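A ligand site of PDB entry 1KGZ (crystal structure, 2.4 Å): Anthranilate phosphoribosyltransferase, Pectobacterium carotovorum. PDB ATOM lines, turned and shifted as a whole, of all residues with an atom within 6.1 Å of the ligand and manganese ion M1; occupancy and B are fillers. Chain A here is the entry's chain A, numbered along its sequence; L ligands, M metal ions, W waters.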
ATOM      1  N   ILE A  89      28.501   7.881  -6.600  1.00  0.00           N
ATOM      2  CA  ILE A  89      27.203   8.479  -6.865  1.00  0.00           C
ATOM      3  C   ILE A  89      26.794   7.784  -8.158  1.00  0.00           C
ATOM      4  O   ILE A  89      27.181   8.194  -9.255  1.00  0.00           O
ATOM      5  CB  ILE A  89      27.332  10.009  -7.058  1.00  0.00           C
ATOM      6  CG1 ILE A  89      26.037  10.591  -7.619  1.00  0.00           C
ATOM      7  CG2 ILE A  89      28.505  10.318  -7.967  1.00  0.00           C
ATOM      8  CD1 ILE A  89      24.819  10.310  -6.774  1.00  0.00           C
ATOM      9  N   VAL A  90      26.019   6.707  -8.022  1.00  0.00           N
ATOM     10  CA  VAL A  90      25.581   5.931  -9.170  1.00  0.00           C
ATOM     11  C   VAL A  90      24.189   5.337  -8.979  1.00  0.00           C
ATOM     12  O   VAL A  90      23.764   5.092  -7.861  1.00  0.00           O
ATOM     13  CB  VAL A  90      26.597   4.788  -9.441  1.00  0.00           C
ATOM     14  CG1 VAL A  90      26.611   3.806  -8.281  1.00  0.00           C
ATOM     15  CG2 VAL A  90      26.255   4.070 -10.744  1.00  0.00           C
ATOM     16  N   GLY A  91      23.493   5.108 -10.082  1.00  0.00           N
ATOM     17  CA  GLY A  91      22.151   4.555 -10.005  1.00  0.00           C
ATOM     18  C   GLY A  91      21.879   3.423 -10.987  1.00  0.00           C
ATOM     19  O   GLY A  91      22.598   3.262 -11.976  1.00  0.00           O
ATOM     20  N   THR A  92      20.841   2.638 -10.707  1.00  0.00           N
ATOM     21  CA  THR A  92      20.457   1.519 -11.562  1.00  0.00           C
ATOM     22  C   THR A  92      20.101   2.009 -12.969  1.00  0.00           C
ATOM     23  O   THR A  92      20.219   1.258 -13.938  1.00  0.00           O
ATOM     24  CB  THR A  92      19.212   0.811 -11.026  1.00  0.00           C
ATOM     25  OG1 THR A  92      18.093   1.710 -11.089  1.00  0.00           O
ATOM     26  CG2 THR A  92      19.429   0.344  -9.592  1.00  0.00           C
ATOM     27  N   GLY A  93      19.657   3.257 -13.053  1.00  0.00           N
ATOM     28  CA  GLY A  93      19.275   3.800 -14.351  1.00  0.00           C
ATOM     29  C   GLY A  93      17.968   3.178 -14.792  1.00  0.00           C
ATOM     30  O   GLY A  93      17.305   2.495 -14.003  1.00  0.00           O
ATOM     31  N   GLY A  94      17.597   3.390 -16.054  1.00  0.00           N
ATOM     32  CA  GLY A  94      16.355   2.836 -16.571  1.00  0.00           C
ATOM     33  C   GLY A  94      15.153   3.180 -15.699  1.00  0.00           C
ATOM     34  O   GLY A  94      14.357   2.303 -15.361  1.00  0.00           O
ATOM     35  N   ASP A  95      15.031   4.449 -15.346  1.00  0.00           N
ATOM     36  CA  ASP A  95      13.932   4.909 -14.505  1.00  0.00           C
ATOM     37  C   ASP A  95      12.650   5.153 -15.317  1.00  0.00           C
ATOM     38  O   ASP A  95      11.573   5.359 -14.758  1.00  0.00           O
ATOM     39  CB  ASP A  95      14.341   6.185 -13.747  1.00  0.00           C
ATOM     40  CG  ASP A  95      15.013   7.227 -14.646  1.00  0.00           C
ATOM     41  OD1 ASP A  95      15.443   8.267 -14.118  1.00  0.00           O
ATOM     42  OD2 ASP A  95      15.094   7.006 -15.882  1.00  0.00           O
ATOM     43  N   GLY A  96      12.779   5.110 -16.643  1.00  0.00           N
ATOM     44  CA  GLY A  96      11.628   5.317 -17.502  1.00  0.00           C
ATOM     45  C   GLY A  96      11.478   6.757 -17.941  1.00  0.00           C
ATOM     46  O   GLY A  96      11.244   7.043 -19.114  1.00  0.00           O
ATOM     47  N   ILE A 100      18.101  14.080 -17.622  1.00  0.00           N
ATOM     48  CA  ILE A 100      19.498  14.370 -17.887  1.00  0.00           C
ATOM     49  C   ILE A 100      20.356  13.503 -16.961  1.00  0.00           C
ATOM     50  O   ILE A 100      19.810  12.831 -16.074  1.00  0.00           O
ATOM     51  CB  ILE A 100      19.821  15.869 -17.671  1.00  0.00           C
ATOM     52  CG1 ILE A 100      19.449  16.275 -16.236  1.00  0.00           C
ATOM     53  CG2 ILE A 100      19.071  16.731 -18.677  1.00  0.00           C
ATOM     54  CD1 ILE A 100      19.902  17.668 -15.857  1.00  0.00           C
ATOM     55  N   ASN A 101      21.664  13.525 -17.158  1.00  0.00           N
ATOM     56  CA  ASN A 101      22.589  12.743 -16.331  1.00  0.00           C
ATOM     57  C   ASN A 101      22.922  13.453 -15.024  1.00  0.00           C
ATOM     58  O   ASN A 101      23.948  14.123 -14.909  1.00  0.00           O
ATOM     59  CB  ASN A 101      23.876  12.465 -17.093  1.00  0.00           C
ATOM     60  CG  ASN A 101      23.668  11.543 -18.283  1.00  0.00           C
ATOM     61  OD1 ASN A 101      24.577  11.331 -19.100  1.00  0.00           O
ATOM     62  ND2 ASN A 101      22.466  10.972 -18.388  1.00  0.00           N
ATOM     63  N   ILE A 102      22.039  13.297 -14.041  1.00  0.00           N
ATOM     64  CA  ILE A 102      22.198  13.919 -12.736  1.00  0.00           C
ATOM     65  C   ILE A 102      23.457  13.474 -11.969  1.00  0.00           C
ATOM     66  O   ILE A 102      24.259  14.319 -11.534  1.00  0.00           O
ATOM     67  CB  ILE A 102      20.947  13.642 -11.865  1.00  0.00           C
ATOM     68  CG1 ILE A 102      19.692  14.211 -12.537  1.00  0.00           C
ATOM     69  CG2 ILE A 102      21.138  14.235 -10.480  1.00  0.00           C
ATOM     70  CD1 ILE A 102      19.696  15.732 -12.692  1.00  0.00           C
ATOM     71  N   SER A 103      23.639  12.161 -11.816  1.00  0.00           N
ATOM     72  CA  SER A 103      24.779  11.611 -11.097  1.00  0.00           C
ATOM     73  C   SER A 103      26.143  12.064 -11.612  1.00  0.00           C
ATOM     74  O   SER A 103      27.032  12.373 -10.817  1.00  0.00           O
ATOM     75  CB  SER A 103      24.706  10.091 -11.104  1.00  0.00           C
ATOM     76  OG  SER A 103      23.537   9.618 -10.453  1.00  0.00           O
ATOM     77  N   THR A 104      26.303  12.106 -12.926  1.00  0.00           N
ATOM     78  CA  THR A 104      27.573  12.502 -13.532  1.00  0.00           C
ATOM     79  C   THR A 104      27.888  13.969 -13.244  1.00  0.00           C
ATOM     80  O   THR A 104      29.050  14.343 -13.003  1.00  0.00           O
ATOM     81  CB  THR A 104      27.544  12.288 -15.069  1.00  0.00           C
ATOM     82  OG1 THR A 104      27.360  10.887 -15.339  1.00  0.00           O
ATOM     83  CG2 THR A 104      28.830  12.747 -15.714  1.00  0.00           C
ATOM     84  N   ALA A 105      26.859  14.796 -13.297  1.00  0.00           N
ATOM     85  CA  ALA A 105      27.023  16.229 -13.030  1.00  0.00           C
ATOM     86  C   ALA A 105      27.294  16.441 -11.539  1.00  0.00           C
ATOM     87  O   ALA A 105      28.127  17.268 -11.156  1.00  0.00           O
ATOM     88  CB  ALA A 105      25.764  16.989 -13.458  1.00  0.00           C
ATOM     89  N   LYS A 119      33.550   7.781  -9.404  1.00  0.00           N
ATOM     90  CA  LYS A 119      32.386   7.213 -10.077  1.00  0.00           C
ATOM     91  C   LYS A 119      32.632   6.032 -11.018  1.00  0.00           C
ATOM     92  O   LYS A 119      33.572   6.011 -11.809  1.00  0.00           O
ATOM     93  CB  LYS A 119      31.622   8.320 -10.821  1.00  0.00           C
ATOM     94  CG  LYS A 119      30.179   7.935 -11.102  1.00  0.00           C
ATOM     95  CD  LYS A 119      29.400   9.028 -11.819  1.00  0.00           C
ATOM     96  CE  LYS A 119      27.990   8.536 -12.086  1.00  0.00           C
ATOM     97  NZ  LYS A 119      28.036   7.125 -12.568  1.00  0.00           N
ATOM     98  N   HIS A 120      31.744   5.050 -10.899  1.00  0.00           N
ATOM     99  CA  HIS A 120      31.768   3.811 -11.673  1.00  0.00           C
ATOM    100  C   HIS A 120      30.553   3.818 -12.598  1.00  0.00           C
ATOM    101  O   HIS A 120      29.509   4.383 -12.246  1.00  0.00           O
ATOM    102  CB  HIS A 120      31.691   2.643 -10.694  1.00  0.00           C
ATOM    103  CG  HIS A 120      31.526   1.302 -11.340  1.00  0.00           C
ATOM    104  ND1 HIS A 120      32.506   0.704 -12.096  1.00  0.00           N
ATOM    105  CD2 HIS A 120      30.493   0.411 -11.290  1.00  0.00           C
ATOM    106  CE1 HIS A 120      32.090  -0.484 -12.496  1.00  0.00           C
ATOM    107  NE2 HIS A 120      30.884  -0.683 -12.019  1.00  0.00           N
ATOM    108  N   GLY A 121      30.683   3.207 -13.766  1.00  0.00           N
ATOM    109  CA  GLY A 121      29.568   3.154 -14.699  1.00  0.00           C
ATOM    110  C   GLY A 121      29.982   3.053 -16.152  1.00  0.00           C
ATOM    111  O   GLY A 121      31.031   3.565 -16.540  1.00  0.00           O
ATOM    112  N   ASN A 122      29.163   2.385 -16.967  1.00  0.00           N
ATOM    113  CA  ASN A 122      29.488   2.225 -18.376  1.00  0.00           C
ATOM    114  C   ASN A 122      28.378   2.642 -19.343  1.00  0.00           C
ATOM    115  O   ASN A 122      27.190   2.507 -19.047  1.00  0.00           O
ATOM    116  CB  ASN A 122      29.926   0.783 -18.686  1.00  0.00           C
ATOM    117  CG  ASN A 122      28.841  -0.234 -18.394  1.00  0.00           C
ATOM    118  OD1 ASN A 122      28.250  -0.245 -17.311  1.00  0.00           O
ATOM    119  ND2 ASN A 122      28.595  -1.125 -19.355  1.00  0.00           N
ATOM    120  N   ARG A 123      28.804   3.147 -20.500  1.00  0.00           N
ATOM    121  CA  ARG A 123      27.918   3.599 -21.567  1.00  0.00           C
ATOM    122  C   ARG A 123      26.620   2.805 -21.700  1.00  0.00           C
ATOM    123  O   ARG A 123      26.604   1.579 -21.505  1.00  0.00           O
ATOM    124  CB  ARG A 123      28.681   3.556 -22.898  1.00  0.00           C
ATOM    125  CG  ARG A 123      29.399   2.241 -23.143  1.00  0.00           C
ATOM    126  CD  ARG A 123      30.053   2.191 -24.526  1.00  0.00           C
ATOM    127  NE  ARG A 123      29.071   2.304 -25.608  1.00  0.00           N
ATOM    128  CZ  ARG A 123      28.089   1.437 -25.828  1.00  0.00           C
ATOM    129  NH1 ARG A 123      27.260   1.638 -26.848  1.00  0.00           N
ATOM    130  NH2 ARG A 123      27.930   0.378 -25.048  1.00  0.00           N
ATOM    131  N   SER A 124      25.538   3.505 -22.019  1.00  0.00           N
ATOM    132  CA  SER A 124      24.223   2.877 -22.193  1.00  0.00           C
ATOM    133  C   SER A 124      24.289   1.679 -23.141  1.00  0.00           C
ATOM    134  O   SER A 124      24.823   1.847 -24.258  1.00  0.00           O
ATOM    135  CB  SER A 124      23.202   3.895 -22.734  1.00  0.00           C
ATOM    136  OG  SER A 124      22.866   4.867 -21.765  1.00  0.00           O
ATOM    137  N   GLY A 131      22.631   8.161 -23.984  1.00  0.00           N
ATOM    138  CA  GLY A 131      22.712   7.620 -22.639  1.00  0.00           C
ATOM    139  C   GLY A 131      23.766   8.326 -21.810  1.00  0.00           C
ATOM    140  O   GLY A 131      23.968   9.537 -21.942  1.00  0.00           O
ATOM    141  N   SER A 132      24.446   7.582 -20.941  1.00  0.00           N
ATOM    142  CA  SER A 132      25.486   8.149 -20.085  1.00  0.00           C
ATOM    143  C   SER A 132      26.869   7.671 -20.492  1.00  0.00           C
ATOM    144  O   SER A 132      27.004   6.812 -21.356  1.00  0.00           O
ATOM    145  CB  SER A 132      25.238   7.767 -18.623  1.00  0.00           C
ATOM    146  OG  SER A 132      26.336   8.169 -17.810  1.00  0.00           O
ATOM    147  N   CYS A 133      27.889   8.227 -19.848  1.00  0.00           N
ATOM    148  CA  CYS A 133      29.274   7.850 -20.123  1.00  0.00           C
ATOM    149  C   CYS A 133      29.690   8.222 -21.549  1.00  0.00           C
ATOM    150  O   CYS A 133      30.880   8.241 -21.870  1.00  0.00           O
ATOM    151  CB  CYS A 133      29.459   6.349 -19.915  1.00  0.00           C
ATOM    152  SG  CYS A 133      31.154   5.769 -20.179  1.00  0.00           S
ATOM    153  N   ASP A 236      15.481   7.617 -10.305  1.00  0.00           N
ATOM    154  CA  ASP A 236      16.383   6.813  -9.485  1.00  0.00           C
ATOM    155  C   ASP A 236      17.424   7.762  -8.902  1.00  0.00           C
ATOM    156  O   ASP A 236      18.627   7.579  -9.069  1.00  0.00           O
ATOM    157  CB  ASP A 236      17.074   5.734 -10.315  1.00  0.00           C
ATOM    158  CG  ASP A 236      17.864   6.303 -11.453  1.00  0.00           C
ATOM    159  OD1 ASP A 236      18.831   5.640 -11.895  1.00  0.00           O
ATOM    160  OD2 ASP A 236      17.527   7.409 -11.918  1.00  0.00           O
ATOM    161  N   GLU A 237      16.917   8.782  -8.218  1.00  0.00           N
ATOM    162  CA  GLU A 237      17.760   9.795  -7.592  1.00  0.00           C
ATOM    163  C   GLU A 237      16.970  10.569  -6.572  1.00  0.00           C
ATOM    164  O   GLU A 237      15.949  10.105  -6.057  1.00  0.00           O
ATOM    165  CB  GLU A 237      18.293  10.741  -8.647  1.00  0.00           C
ATOM    166  CG  GLU A 237      19.447  10.168  -9.415  1.00  0.00           C
ATOM    167  CD  GLU A 237      19.587  10.784 -10.772  1.00  0.00           C
ATOM    168  OE1 GLU A 237      20.537  10.405 -11.475  1.00  0.00           O
ATOM    169  OE2 GLU A 237      18.758  11.642 -11.126  1.00  0.00           O
HETATM  170  C1  LIG L   1      22.604   5.199 -14.971  1.00  0.00           C
HETATM  171  C2  LIG L   1      23.326   3.898 -15.331  1.00  0.00           C
HETATM  172  C3  LIG L   1      23.058   3.502 -16.676  1.00  0.00           C
HETATM  173  C4  LIG L   1      21.916   4.265 -17.084  1.00  0.00           C
HETATM  174  C5  LIG L   1      20.646   3.634 -17.506  1.00  0.00           C
HETATM  175  O1  LIG L   1      23.576   6.318 -14.993  1.00  0.00           O
HETATM  176  O2  LIG L   1      24.727   4.028 -15.046  1.00  0.00           O
HETATM  177  O3  LIG L   1      24.224   3.792 -17.487  1.00  0.00           O
HETATM  178  O4  LIG L   1      21.667   5.307 -15.989  1.00  0.00           O
HETATM  179  O5  LIG L   1      19.614   4.561 -17.861  1.00  0.00           O
HETATM  180  P1  LIG L   1      18.655   4.429 -19.185  1.00  0.00           P
HETATM  181  O6  LIG L   1      17.410   5.266 -18.937  1.00  0.00           O
HETATM  182  O7  LIG L   1      19.442   4.891 -20.404  1.00  0.00           O
HETATM  183  O8  LIG L   1      18.339   2.934 -19.214  1.00  0.00           O
HETATM  184  P2  LIG L   1      24.171   6.944 -13.610  1.00  0.00           P
HETATM  185  O9  LIG L   1      23.584   6.253 -12.444  1.00  0.00           O
HETATM  186  O10 LIG L   1      25.652   6.892 -13.687  1.00  0.00           O
HETATM  187  O11 LIG L   1      23.593   8.439 -13.703  1.00  0.00           O
HETATM  188  P3  LIG L   1      23.937   9.601 -14.850  1.00  0.00           P
HETATM  189  O12 LIG L   1      22.653   9.693 -15.676  1.00  0.00           O
HETATM  190  O13 LIG L   1      25.118   9.114 -15.635  1.00  0.00           O
HETATM  191  O14 LIG L   1      24.220  10.856 -14.080  1.00  0.00           O
HETATM  192 MN    MN M   1      21.963   8.683 -12.016  1.00  0.00          MN
HETATM  193 MN    MN M   2      18.920   8.501 -13.218  1.00  0.00          MN
HETATM  194  O   HOH W   1      22.445   7.260 -17.634  1.00  0.00           O
HETATM  195  O   HOH W   2      20.230   9.933 -14.392  1.00  0.00           O
HETATM  196  O   HOH W   3      20.751   6.658 -12.676  1.00  0.00           O
HETATM  197  O   HOH W   4      21.394   7.606  -9.936  1.00  0.00           O
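The backbone NH (N) of Ser 103 is in hydrogen-bond range of an oxygen (O14) of the ligand. O10 of the ligand is in salt-bridge range of NZ of Lys 119 (2.6 Å). The side-chain hydroxyl of Ser 132 sits at hydrogen-bond distance from an oxygen (O13) of the ligand. N of Ile 102 sits at hydrogen-bond distance from O14 of the ligand. ND2 of Asn 101 sits at hydrogen-bond distance from O12 of the ligand, 3.0 Å away. An oxygen (O5) of the ligand is in hydrogen-bond range of the backbone NH (N) of Gly 94, at 3.0 Å. An oxygen (O13) of the ligand lies within hydrogen-bond range of the side-chain hydroxyl of Thr 104, 2.9 Å away. The backbone NH (N) of Gly 91 is in hydrogen-bond range of an oxygen (O9) of the ligand. The backbone NH (N) of Thr 104 is in hydrogen-bond range of an oxygen (O14) of the ligand (2.7 Å).
N of Gly 93 is in hydrogen-bond range of OD1 of Asp 236 (2.8 Å). O of Gly 131 lies close to OD1 of Asn 101 (3.4 Å). The backbone NH (N) of Ser 132 is in hydrogen-bond range of the side-chain hydroxyl (OG) of Ser 124, 3.2 Å away.
Val 90 touches the ligand. CA of Gly 93 touches O4 of the ligand, at 3.3 Å. Asn 122 touches the ligand (O to O3, 3.6 Å). Ser 124 touches the ligand (OG to O7, 3.7 Å). Hydrophobic or aromatic side chains that line the ligand: Val 90.
Of the 25 residues printed, 2 come within 4 Å of manganese ion M1. The nearest printed residue that does not touch manganese ion M1 is Gly 91 (4.3 Å).
Manganese ion M1 is bound by OE1 of Glu 237, O11 of the ligand, OG of Ser 103, water W4 and water W3.
Water W4 lies within hydrogen-bond range of the backbone carbonyl oxygen (O) of Asp 236 (2.9 Å) and the backbone NH (N) of Gly 91 (3.3 Å). Water W2 lies within hydrogen-bond range of an oxygen (O12) of the ligand (2.8 Å) and the backbone carbonyl oxygen (O) of Ile 100 (3.4 Å).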
